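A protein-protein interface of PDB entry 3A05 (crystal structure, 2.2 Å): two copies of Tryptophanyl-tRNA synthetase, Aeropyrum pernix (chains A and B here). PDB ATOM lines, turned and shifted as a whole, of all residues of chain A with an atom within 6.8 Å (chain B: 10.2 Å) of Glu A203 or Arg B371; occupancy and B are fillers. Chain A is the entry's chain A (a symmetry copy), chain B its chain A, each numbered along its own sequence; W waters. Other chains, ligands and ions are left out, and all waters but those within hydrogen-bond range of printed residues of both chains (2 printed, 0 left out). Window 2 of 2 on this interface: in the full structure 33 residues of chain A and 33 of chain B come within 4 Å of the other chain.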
ATOM      1  N   GLU A 147     -16.435   6.916  10.519  1.00  0.00           N
ATOM      2  CA  GLU A 147     -14.969   6.733  10.428  1.00  0.00           C
ATOM      3  C   GLU A 147     -14.600   6.648   8.979  1.00  0.00           C
ATOM      4  O   GLU A 147     -14.915   5.649   8.335  1.00  0.00           O
ATOM      5  CB  GLU A 147     -14.607   5.427  11.165  1.00  0.00           C
ATOM      6  CG  GLU A 147     -13.086   5.232  11.355  1.00  0.00           C
ATOM      7  CD  GLU A 147     -12.729   4.316  12.517  1.00  0.00           C
ATOM      8  OE1 GLU A 147     -13.403   4.344  13.608  1.00  0.00           O
ATOM      9  OE2 GLU A 147     -11.744   3.562  12.334  1.00  0.00           O
ATOM     10  N   ARG A 154      -4.285   3.143   6.361  1.00  0.00           N
ATOM     11  CA  ARG A 154      -5.246   2.563   7.312  1.00  0.00           C
ATOM     12  C   ARG A 154      -4.494   1.719   8.381  1.00  0.00           C
ATOM     13  O   ARG A 154      -4.984   1.570   9.499  1.00  0.00           O
ATOM     14  CB  ARG A 154      -6.273   1.740   6.539  1.00  0.00           C
ATOM     15  CG  ARG A 154      -7.367   1.153   7.457  1.00  0.00           C
ATOM     16  CD  ARG A 154      -7.970   2.318   8.345  1.00  0.00           C
ATOM     17  NE  ARG A 154      -9.286   1.844   8.745  1.00  0.00           N
ATOM     18  CZ  ARG A 154      -9.971   2.362   9.743  1.00  0.00           C
ATOM     19  NH1 ARG A 154      -9.483   3.393  10.389  1.00  0.00           N
ATOM     20  NH2 ARG A 154     -11.099   1.789  10.122  1.00  0.00           N
ATOM     21  N   PRO A 157      -2.500  -3.737  10.719  1.00  0.00           N
ATOM     22  CA  PRO A 157      -3.368  -4.958  10.818  1.00  0.00           C
ATOM     23  C   PRO A 157      -4.305  -5.112   9.636  1.00  0.00           C
ATOM     24  O   PRO A 157      -4.652  -6.225   9.218  1.00  0.00           O
ATOM     25  CB  PRO A 157      -4.210  -4.740  12.096  1.00  0.00           C
ATOM     26  CG  PRO A 157      -3.460  -3.580  12.820  1.00  0.00           C
ATOM     27  CD  PRO A 157      -2.683  -2.794  11.837  1.00  0.00           C
ATOM     28  N   ARG A 160      -2.077  -6.372   6.800  1.00  0.00           N
ATOM     29  CA  ARG A 160      -1.740  -7.799   7.042  1.00  0.00           C
ATOM     30  C   ARG A 160      -2.819  -8.671   6.471  1.00  0.00           C
ATOM     31  O   ARG A 160      -2.530  -9.710   5.836  1.00  0.00           O
ATOM     32  CB  ARG A 160      -1.533  -8.089   8.548  1.00  0.00           C
ATOM     33  CG  ARG A 160      -1.054  -9.546   8.754  1.00  0.00           C
ATOM     34  CD  ARG A 160      -0.631  -9.763  10.217  1.00  0.00           C
ATOM     35  NE  ARG A 160       0.272  -8.724  10.749  1.00  0.00           N
ATOM     36  CZ  ARG A 160       0.080  -8.159  11.925  1.00  0.00           C
ATOM     37  NH1 ARG A 160      -0.939  -8.570  12.654  1.00  0.00           N
ATOM     38  NH2 ARG A 160       0.886  -7.212  12.395  1.00  0.00           N
ATOM     39  N   HIS A 198     -11.764  -5.855   7.735  1.00  0.00           N
ATOM     40  CA  HIS A 198     -10.824  -5.365   8.794  1.00  0.00           C
ATOM     41  C   HIS A 198     -11.451  -4.769  10.035  1.00  0.00           C
ATOM     42  O   HIS A 198     -10.812  -4.705  11.127  1.00  0.00           O
ATOM     43  CB  HIS A 198      -9.808  -4.344   8.248  1.00  0.00           C
ATOM     44  CG  HIS A 198     -10.348  -2.933   8.181  1.00  0.00           C
ATOM     45  ND1 HIS A 198     -11.353  -2.562   7.310  1.00  0.00           N
ATOM     46  CD2 HIS A 198     -10.052  -1.827   8.903  1.00  0.00           C
ATOM     47  CE1 HIS A 198     -11.627  -1.280   7.468  1.00  0.00           C
ATOM     48  NE2 HIS A 198     -10.869  -0.808   8.442  1.00  0.00           N
ATOM     49  N   VAL A 199     -12.668  -4.270   9.890  1.00  0.00           N
ATOM     50  CA  VAL A 199     -13.360  -3.645  11.040  1.00  0.00           C
ATOM     51  C   VAL A 199     -13.691  -4.654  12.147  1.00  0.00           C
ATOM     52  O   VAL A 199     -13.971  -4.272  13.299  1.00  0.00           O
ATOM     53  CB  VAL A 199     -14.673  -2.893  10.616  1.00  0.00           C
ATOM     54  CG1 VAL A 199     -14.370  -1.824   9.540  1.00  0.00           C
ATOM     55  CG2 VAL A 199     -15.737  -3.875  10.110  1.00  0.00           C
ATOM     56  N   GLN A 200     -13.602  -5.932  11.804  1.00  0.00           N
ATOM     57  CA  GLN A 200     -13.801  -7.012  12.780  1.00  0.00           C
ATOM     58  C   GLN A 200     -12.555  -7.124  13.707  1.00  0.00           C
ATOM     59  O   GLN A 200     -12.686  -7.567  14.806  1.00  0.00           O
ATOM     60  CB  GLN A 200     -14.045  -8.334  12.062  1.00  0.00           C
ATOM     61  CG  GLN A 200     -15.083  -8.338  10.942  1.00  0.00           C
ATOM     62  CD  GLN A 200     -15.527  -9.772  10.655  1.00  0.00           C
ATOM     63  OE1 GLN A 200     -15.562 -10.597  11.565  1.00  0.00           O
ATOM     64  NE2 GLN A 200     -15.920 -10.060   9.442  1.00  0.00           N
ATOM     65  N   LEU A 201     -11.374  -6.648  13.284  1.00  0.00           N
ATOM     66  CA  LEU A 201     -10.162  -6.692  14.135  1.00  0.00           C
ATOM     67  C   LEU A 201     -10.326  -5.757  15.285  1.00  0.00           C
ATOM     68  O   LEU A 201     -10.924  -4.690  15.133  1.00  0.00           O
ATOM     69  CB  LEU A 201      -8.899  -6.263  13.377  1.00  0.00           C
ATOM     70  CG  LEU A 201      -8.697  -7.110  12.112  1.00  0.00           C
ATOM     71  CD1 LEU A 201      -7.608  -6.544  11.257  1.00  0.00           C
ATOM     72  CD2 LEU A 201      -8.403  -8.623  12.501  1.00  0.00           C
ATOM     73  N   ASP A 202      -9.742  -6.128  16.413  1.00  0.00           N
ATOM     74  CA  ASP A 202      -9.843  -5.404  17.648  1.00  0.00           C
ATOM     75  C   ASP A 202      -9.255  -4.043  17.504  1.00  0.00           C
ATOM     76  O   ASP A 202      -9.750  -3.080  18.122  1.00  0.00           O
ATOM     77  CB  ASP A 202      -9.156  -6.207  18.800  1.00  0.00           C
ATOM     78  CG  ASP A 202      -9.838  -7.581  19.008  1.00  0.00           C
ATOM     79  OD1 ASP A 202     -11.082  -7.665  18.800  1.00  0.00           O
ATOM     80  OD2 ASP A 202      -9.164  -8.577  19.317  1.00  0.00           O
ATOM     81  N   GLU A 203      -8.235  -3.919  16.672  1.00  0.00           N
ATOM     82  CA  GLU A 203      -7.604  -2.592  16.499  1.00  0.00           C
ATOM     83  C   GLU A 203      -8.482  -1.547  15.786  1.00  0.00           C
ATOM     84  O   GLU A 203      -8.155  -0.361  15.788  1.00  0.00           O
ATOM     85  CB  GLU A 203      -6.304  -2.712  15.746  1.00  0.00           C
ATOM     86  CG  GLU A 203      -5.230  -3.576  16.444  1.00  0.00           C
ATOM     87  CD  GLU A 203      -5.259  -5.050  16.028  1.00  0.00           C
ATOM     88  OE1 GLU A 203      -6.284  -5.559  15.544  1.00  0.00           O
ATOM     89  OE2 GLU A 203      -4.230  -5.748  16.214  1.00  0.00           O
ATOM     90  N   TYR A 204      -9.585  -1.986  15.185  1.00  0.00           N
ATOM     91  CA  TYR A 204     -10.426  -1.048  14.519  1.00  0.00           C
ATOM     92  C   TYR A 204     -11.792  -1.004  15.188  1.00  0.00           C
ATOM     93  O   TYR A 204     -12.703  -0.450  14.619  1.00  0.00           O
ATOM     94  CB  TYR A 204     -10.546  -1.367  12.986  1.00  0.00           C
ATOM     95  CG  TYR A 204      -9.212  -1.258  12.287  1.00  0.00           C
ATOM     96  CD1 TYR A 204      -8.623   0.011  12.043  1.00  0.00           C
ATOM     97  CD2 TYR A 204      -8.493  -2.423  11.929  1.00  0.00           C
ATOM     98  CE1 TYR A 204      -7.378   0.111  11.419  1.00  0.00           C
ATOM     99  CE2 TYR A 204      -7.247  -2.329  11.321  1.00  0.00           C
ATOM    100  CZ  TYR A 204      -6.687  -1.068  11.081  1.00  0.00           C
ATOM    101  OH  TYR A 204      -5.491  -0.986  10.448  1.00  0.00           O
ATOM    102  N   GLY A 205     -11.934  -1.622  16.376  1.00  0.00           N
ATOM    103  CA  GLY A 205     -13.208  -1.580  17.137  1.00  0.00           C
ATOM    104  C   GLY A 205     -13.854  -2.936  17.374  1.00  0.00           C
ATOM    105  O   GLY A 205     -14.788  -3.040  18.164  1.00  0.00           O
ATOM    106  N   GLY A 206     -13.362  -3.980  16.685  1.00  0.00           N
ATOM    107  CA  GLY A 206     -13.944  -5.311  16.801  1.00  0.00           C
ATOM    108  C   GLY A 206     -15.391  -5.499  16.409  1.00  0.00           C
ATOM    109  O   GLY A 206     -16.138  -6.158  17.134  1.00  0.00           O
ATOM    110  N   VAL A 235      -6.514 -18.562  11.549  1.00  0.00           N
ATOM    111  CA  VAL A 235      -5.481 -17.533  11.431  1.00  0.00           C
ATOM    112  C   VAL A 235      -6.039 -16.287  12.049  1.00  0.00           C
ATOM    113  O   VAL A 235      -5.465 -15.715  12.967  1.00  0.00           O
ATOM    114  CB  VAL A 235      -5.180 -17.306   9.952  1.00  0.00           C
ATOM    115  CG1 VAL A 235      -3.950 -16.525   9.777  1.00  0.00           C
ATOM    116  CG2 VAL A 235      -5.096 -18.637   9.248  1.00  0.00           C
ATOM    117  N   VAL A 236      -7.238 -15.916  11.591  1.00  0.00           N
ATOM    118  CA  VAL A 236      -7.964 -14.871  12.270  1.00  0.00           C
ATOM    119  C   VAL A 236      -9.455 -15.176  12.089  1.00  0.00           C
ATOM    120  O   VAL A 236      -9.967 -15.524  10.977  1.00  0.00           O
ATOM    121  CB  VAL A 236      -7.434 -13.401  11.837  1.00  0.00           C
ATOM    122  CG1 VAL A 236      -7.278 -13.300  10.357  1.00  0.00           C
ATOM    123  CG2 VAL A 236      -8.314 -12.272  12.354  1.00  0.00           C
ATOM    124  N   ASP B 110       7.869 -13.536   6.190  1.00  0.00           N
ATOM    125  CA  ASP B 110       6.781 -14.323   6.747  1.00  0.00           C
ATOM    126  C   ASP B 110       5.437 -14.171   5.991  1.00  0.00           C
ATOM    127  O   ASP B 110       4.589 -15.116   6.010  1.00  0.00           O
ATOM    128  CB  ASP B 110       6.599 -13.930   8.220  1.00  0.00           C
ATOM    129  CG  ASP B 110       5.933 -12.543   8.406  1.00  0.00           C
ATOM    130  OD1 ASP B 110       6.338 -11.555   7.739  1.00  0.00           O
ATOM    131  OD2 ASP B 110       5.027 -12.444   9.271  1.00  0.00           O
ATOM    132  N   ARG B 121       1.511 -19.259  10.791  1.00  0.00           N
ATOM    133  CA  ARG B 121       1.942 -17.985  11.363  1.00  0.00           C
ATOM    134  C   ARG B 121       2.865 -18.190  12.564  1.00  0.00           C
ATOM    135  O   ARG B 121       3.937 -17.613  12.641  1.00  0.00           O
ATOM    136  CB  ARG B 121       0.710 -17.104  11.740  1.00  0.00           C
ATOM    137  CG  ARG B 121      -0.253 -16.843  10.519  1.00  0.00           C
ATOM    138  CD  ARG B 121       0.457 -15.858   9.487  1.00  0.00           C
ATOM    139  NE  ARG B 121       0.645 -14.581  10.124  1.00  0.00           N
ATOM    140  CZ  ARG B 121       1.645 -13.754   9.923  1.00  0.00           C
ATOM    141  NH1 ARG B 121       2.637 -14.096   9.122  1.00  0.00           N
ATOM    142  NH2 ARG B 121       1.636 -12.595  10.528  1.00  0.00           N
ATOM    143  N   GLU B 122       2.401 -18.955  13.547  1.00  0.00           N
ATOM    144  CA  GLU B 122       3.170 -19.197  14.772  1.00  0.00           C
ATOM    145  C   GLU B 122       4.550 -19.808  14.432  1.00  0.00           C
ATOM    146  O   GLU B 122       5.569 -19.400  14.964  1.00  0.00           O
ATOM    147  CB  GLU B 122       2.424 -20.172  15.711  1.00  0.00           C
ATOM    148  CG  GLU B 122       2.964 -20.087  17.127  1.00  0.00           C
ATOM    149  CD  GLU B 122       2.445 -21.189  18.093  1.00  0.00           C
ATOM    150  OE1 GLU B 122       1.605 -22.043  17.692  1.00  0.00           O
ATOM    151  OE2 GLU B 122       2.888 -21.182  19.282  1.00  0.00           O
ATOM    152  N   VAL B 125       7.014 -17.429  12.596  1.00  0.00           N
ATOM    153  CA  VAL B 125       7.558 -16.471  13.581  1.00  0.00           C
ATOM    154  C   VAL B 125       8.604 -17.111  14.522  1.00  0.00           C
ATOM    155  O   VAL B 125       9.661 -16.542  14.767  1.00  0.00           O
ATOM    156  CB  VAL B 125       6.429 -15.831  14.443  1.00  0.00           C
ATOM    157  CG1 VAL B 125       7.013 -15.077  15.658  1.00  0.00           C
ATOM    158  CG2 VAL B 125       5.568 -14.818  13.590  1.00  0.00           C
ATOM    159  N   PHE B 150       9.523  -8.062  10.282  1.00  0.00           N
ATOM    160  CA  PHE B 150       8.608  -8.965   9.586  1.00  0.00           C
ATOM    161  C   PHE B 150       7.844  -8.231   8.488  1.00  0.00           C
ATOM    162  O   PHE B 150       7.350  -7.076   8.721  1.00  0.00           O
ATOM    163  CB  PHE B 150       7.545  -9.516  10.583  1.00  0.00           C
ATOM    164  CG  PHE B 150       8.113 -10.448  11.622  1.00  0.00           C
ATOM    165  CD1 PHE B 150       8.291 -11.795  11.337  1.00  0.00           C
ATOM    166  CD2 PHE B 150       8.493  -9.976  12.876  1.00  0.00           C
ATOM    167  CE1 PHE B 150       8.844 -12.690  12.317  1.00  0.00           C
ATOM    168  CE2 PHE B 150       9.040 -10.891  13.879  1.00  0.00           C
ATOM    169  CZ  PHE B 150       9.219 -12.228  13.558  1.00  0.00           C
ATOM    170  N   THR B 152       5.033  -8.731   7.675  1.00  0.00           N
ATOM    171  CA  THR B 152       3.655  -8.549   8.038  1.00  0.00           C
ATOM    172  C   THR B 152       3.587  -7.587   9.182  1.00  0.00           C
ATOM    173  O   THR B 152       2.524  -7.382   9.741  1.00  0.00           O
ATOM    174  CB  THR B 152       2.929  -9.866   8.424  1.00  0.00           C
ATOM    175  OG1 THR B 152       3.533 -10.386   9.587  1.00  0.00           O
ATOM    176  CG2 THR B 152       2.933 -10.851   7.338  1.00  0.00           C
ATOM    177  N   ASN B 153       4.708  -6.988   9.555  1.00  0.00           N
ATOM    178  CA  ASN B 153       4.624  -6.063  10.672  1.00  0.00           C
ATOM    179  C   ASN B 153       5.449  -4.822  10.524  1.00  0.00           C
ATOM    180  O   ASN B 153       6.104  -4.379  11.464  1.00  0.00           O
ATOM    181  CB  ASN B 153       4.984  -6.713  11.982  1.00  0.00           C
ATOM    182  CG  ASN B 153       4.297  -6.019  13.155  1.00  0.00           C
ATOM    183  OD1 ASN B 153       3.122  -5.582  13.028  1.00  0.00           O
ATOM    184  ND2 ASN B 153       4.990  -5.901  14.280  1.00  0.00           N
ATOM    185  N   ARG B 154       5.478  -4.256   9.358  1.00  0.00           N
ATOM    186  CA  ARG B 154       6.538  -3.275   9.078  1.00  0.00           C
ATOM    187  C   ARG B 154       5.929  -1.847   8.987  1.00  0.00           C
ATOM    188  O   ARG B 154       6.622  -0.867   9.257  1.00  0.00           O
ATOM    189  CB  ARG B 154       7.263  -3.680   7.799  1.00  0.00           C
ATOM    190  CG  ARG B 154       8.444  -2.740   7.470  1.00  0.00           C
ATOM    191  CD  ARG B 154       9.365  -2.607   8.752  1.00  0.00           C
ATOM    192  NE  ARG B 154      10.666  -2.199   8.241  1.00  0.00           N
ATOM    193  CZ  ARG B 154      11.607  -1.670   8.994  1.00  0.00           C
ATOM    194  NH1 ARG B 154      11.402  -1.544  10.283  1.00  0.00           N
ATOM    195  NH2 ARG B 154      12.708  -1.209   8.428  1.00  0.00           N
ATOM    196  N   VAL B 367      12.667  -7.982  18.030  1.00  0.00           N
ATOM    197  CA  VAL B 367      11.554  -7.820  17.104  1.00  0.00           C
ATOM    198  C   VAL B 367      10.236  -7.827  17.825  1.00  0.00           C
ATOM    199  O   VAL B 367      10.131  -8.358  18.946  1.00  0.00           O
ATOM    200  CB  VAL B 367      11.542  -8.915  16.007  1.00  0.00           C
ATOM    201  CG1 VAL B 367      12.756  -8.769  15.102  1.00  0.00           C
ATOM    202  CG2 VAL B 367      11.440 -10.339  16.607  1.00  0.00           C
ATOM    203  N   GLU B 368       9.247  -7.205  17.177  1.00  0.00           N
ATOM    204  CA  GLU B 368       7.876  -7.297  17.588  1.00  0.00           C
ATOM    205  C   GLU B 368       7.200  -8.205  16.608  1.00  0.00           C
ATOM    206  O   GLU B 368       7.085  -7.875  15.409  1.00  0.00           O
ATOM    207  CB  GLU B 368       7.218  -5.916  17.579  1.00  0.00           C
ATOM    208  CG  GLU B 368       5.823  -5.909  18.246  1.00  0.00           C
ATOM    209  CD  GLU B 368       5.147  -4.523  18.157  1.00  0.00           C
ATOM    210  OE1 GLU B 368       5.692  -3.578  18.783  1.00  0.00           O
ATOM    211  OE2 GLU B 368       4.093  -4.397  17.450  1.00  0.00           O
ATOM    212  N   PRO B 369       6.788  -9.385  17.090  1.00  0.00           N
ATOM    213  CA  PRO B 369       6.157 -10.381  16.235  1.00  0.00           C
ATOM    214  C   PRO B 369       4.736  -9.871  15.922  1.00  0.00           C
ATOM    215  O   PRO B 369       4.139  -9.233  16.740  1.00  0.00           O
ATOM    216  CB  PRO B 369       6.060 -11.630  17.148  1.00  0.00           C
ATOM    217  CG  PRO B 369       6.964 -11.335  18.288  1.00  0.00           C
ATOM    218  CD  PRO B 369       7.014  -9.890  18.458  1.00  0.00           C
ATOM    219  N   PRO B 370       4.191 -10.225  14.765  1.00  0.00           N
ATOM    220  CA  PRO B 370       2.832  -9.799  14.480  1.00  0.00           C
ATOM    221  C   PRO B 370       1.809 -10.509  15.410  1.00  0.00           C
ATOM    222  O   PRO B 370       2.022 -11.679  15.785  1.00  0.00           O
ATOM    223  CB  PRO B 370       2.663 -10.206  13.032  1.00  0.00           C
ATOM    224  CG  PRO B 370       3.600 -11.496  12.901  1.00  0.00           C
ATOM    225  CD  PRO B 370       4.796 -11.043  13.691  1.00  0.00           C
ATOM    226  N   ARG B 371       0.725  -9.807  15.788  1.00  0.00           N
ATOM    227  CA  ARG B 371      -0.418 -10.352  16.545  1.00  0.00           C
ATOM    228  C   ARG B 371      -1.096 -11.572  15.925  1.00  0.00           C
ATOM    229  O   ARG B 371      -1.635 -12.376  16.698  1.00  0.00           O
ATOM    230  CB  ARG B 371      -1.540  -9.274  16.733  1.00  0.00           C
ATOM    231  CG  ARG B 371      -1.746  -8.554  18.082  1.00  0.00           C
ATOM    232  CD  ARG B 371      -3.308  -8.495  18.534  1.00  0.00           C
ATOM    233  NE  ARG B 371      -4.297  -7.989  17.544  1.00  0.00           N
ATOM    234  CZ  ARG B 371      -5.339  -8.663  17.023  1.00  0.00           C
ATOM    235  NH1 ARG B 371      -5.600  -9.921  17.383  1.00  0.00           N
ATOM    236  NH2 ARG B 371      -6.166  -8.070  16.130  1.00  0.00           N
ATOM    237  N   PHE B 372      -1.200 -11.696  14.585  1.00  0.00           N
ATOM    238  CA  PHE B 372      -1.844 -12.854  13.953  1.00  0.00           C
ATOM    239  C   PHE B 372      -1.168 -13.140  12.593  1.00  0.00           C
ATOM    240  O   PHE B 372      -0.383 -12.224  12.230  1.00  0.00           O
ATOM    241  CB  PHE B 372      -3.347 -12.609  13.739  1.00  0.00           C
ATOM    242  CG  PHE B 372      -3.681 -11.395  12.880  1.00  0.00           C
ATOM    243  CD1 PHE B 372      -4.020 -10.169  13.482  1.00  0.00           C
ATOM    244  CD2 PHE B 372      -3.753 -11.504  11.505  1.00  0.00           C
ATOM    245  CE1 PHE B 372      -4.381  -9.023  12.700  1.00  0.00           C
ATOM    246  CE2 PHE B 372      -4.135 -10.398  10.697  1.00  0.00           C
ATOM    247  CZ  PHE B 372      -4.427  -9.143  11.297  1.00  0.00           C
HETATM  248  O   HOH W   1      -8.658  -9.064  16.327  1.00  0.00           O
HETATM  249  O   HOH W   2       0.837  -6.767  15.369  1.00  0.00           O
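The guanidinium group (NH2) of Arg B371 is in salt-bridge range of the side-chain carboxylate (OE1) of Glu A203 (2.6 Å).
The guanidinium group of Arg A160 lies within hydrogen-bond range of the backbone carbonyl oxygen of Thr B152, at 2.8 Å.
The side-chain amide oxygen (OD1) of Asn B153 is in hydrogen-bond range of the guanidinium group (NH2) of Arg A160 (2.8 Å).
The side-chain amide nitrogen (ND2) of Asn B153 sits at hydrogen-bond distance from the backbone carbonyl oxygen (O) of Glu B368 (3.1 Å).
The side-chain carboxylate (OD2) of Asp B110 is in hydrogen-bond range of the side-chain hydroxyl (OG1) of Thr B152 (2.6 Å).
The guanidinium group (NH1) of Arg B121 is in salt-bridge range of the side-chain carboxylate (OD2) of Asp B110.
The side-chain hydroxyl of Thr B152 is in hydrogen-bond range of the guanidinium group of Arg B121 (3.1 Å).
The guanidinium group (NH2) of Arg B121 is in hydrogen-bond range of the backbone carbonyl oxygen (O) of Phe B372, 2.7 Å away.
Water W1 bridges NH2 of Arg B371 (2.7 Å) and OD2 of Asp A202 (3.1 Å).
Water W2 lies within hydrogen-bond range of the guanidinium group (NH2) of Arg A160 (3.0 Å), the backbone NH (N) of Arg B371 (3.1 Å) and the side-chain amide oxygen (OD1) of Asn B153 (3.5 Å).
Of the printed residues of chain B, Glu A203 touches Arg B371.
Of chain A, only Arg A160 (3.8 Å) and Glu A203 (2.6 Å) come within 4 Å of Arg B371.
No residue of chain B comes within 4 Å of Leu A201.
No residue of chain B comes within 4 Å of Asp A202.
Of the printed residues of chain A, Pro B370 touches Arg A160.
Printed residues of chain B within 4 Å of Val A235: Arg B121 (3.8 Å) and Phe B372 (3.8 Å).
Of the printed residues of chain B, Arg A160 touches Arg B121 (3.6 Å), Thr B152 (2.8 Å), Asn B153 (2.8 Å), Pro B370 (3.5 Å), Arg B371 (3.8 Å) and Phe B372 (3.2 Å).
The nearest residue of chain B that does not touch Glu A203 is Phe B372 (4.8 Å).
The nearest residue of chain A that does not touch Arg B371 is Asp A202 (4.1 Å).
Among the printed residues, pairs that only touch across the chains: Arg A160 with Phe B372 (3.2 Å), Arg A160 with Pro B370 (3.5 Å), Pro A157 with Phe B372 (3.6 Å), Arg A160 with Arg B121 (3.6 Å), Arg A160 with Arg B371 (3.8 Å), Val A235 with Arg B121 (3.8 Å) and Val A235 with Phe B372 (3.8 Å).
Position printed for both chains: 154.
Of the 14 printed residues of chain B, 6 touch a printed residue of chain A.
Printed residues of chain B that touch a printed residue of chain A: Arg B121, Thr B152, Asn B153, Pro B370, Arg B371 and Phe B372.
Hydrophobic or aromatic side chains of chain B that line the printed part of chain A: Pro B370 and Phe B372.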
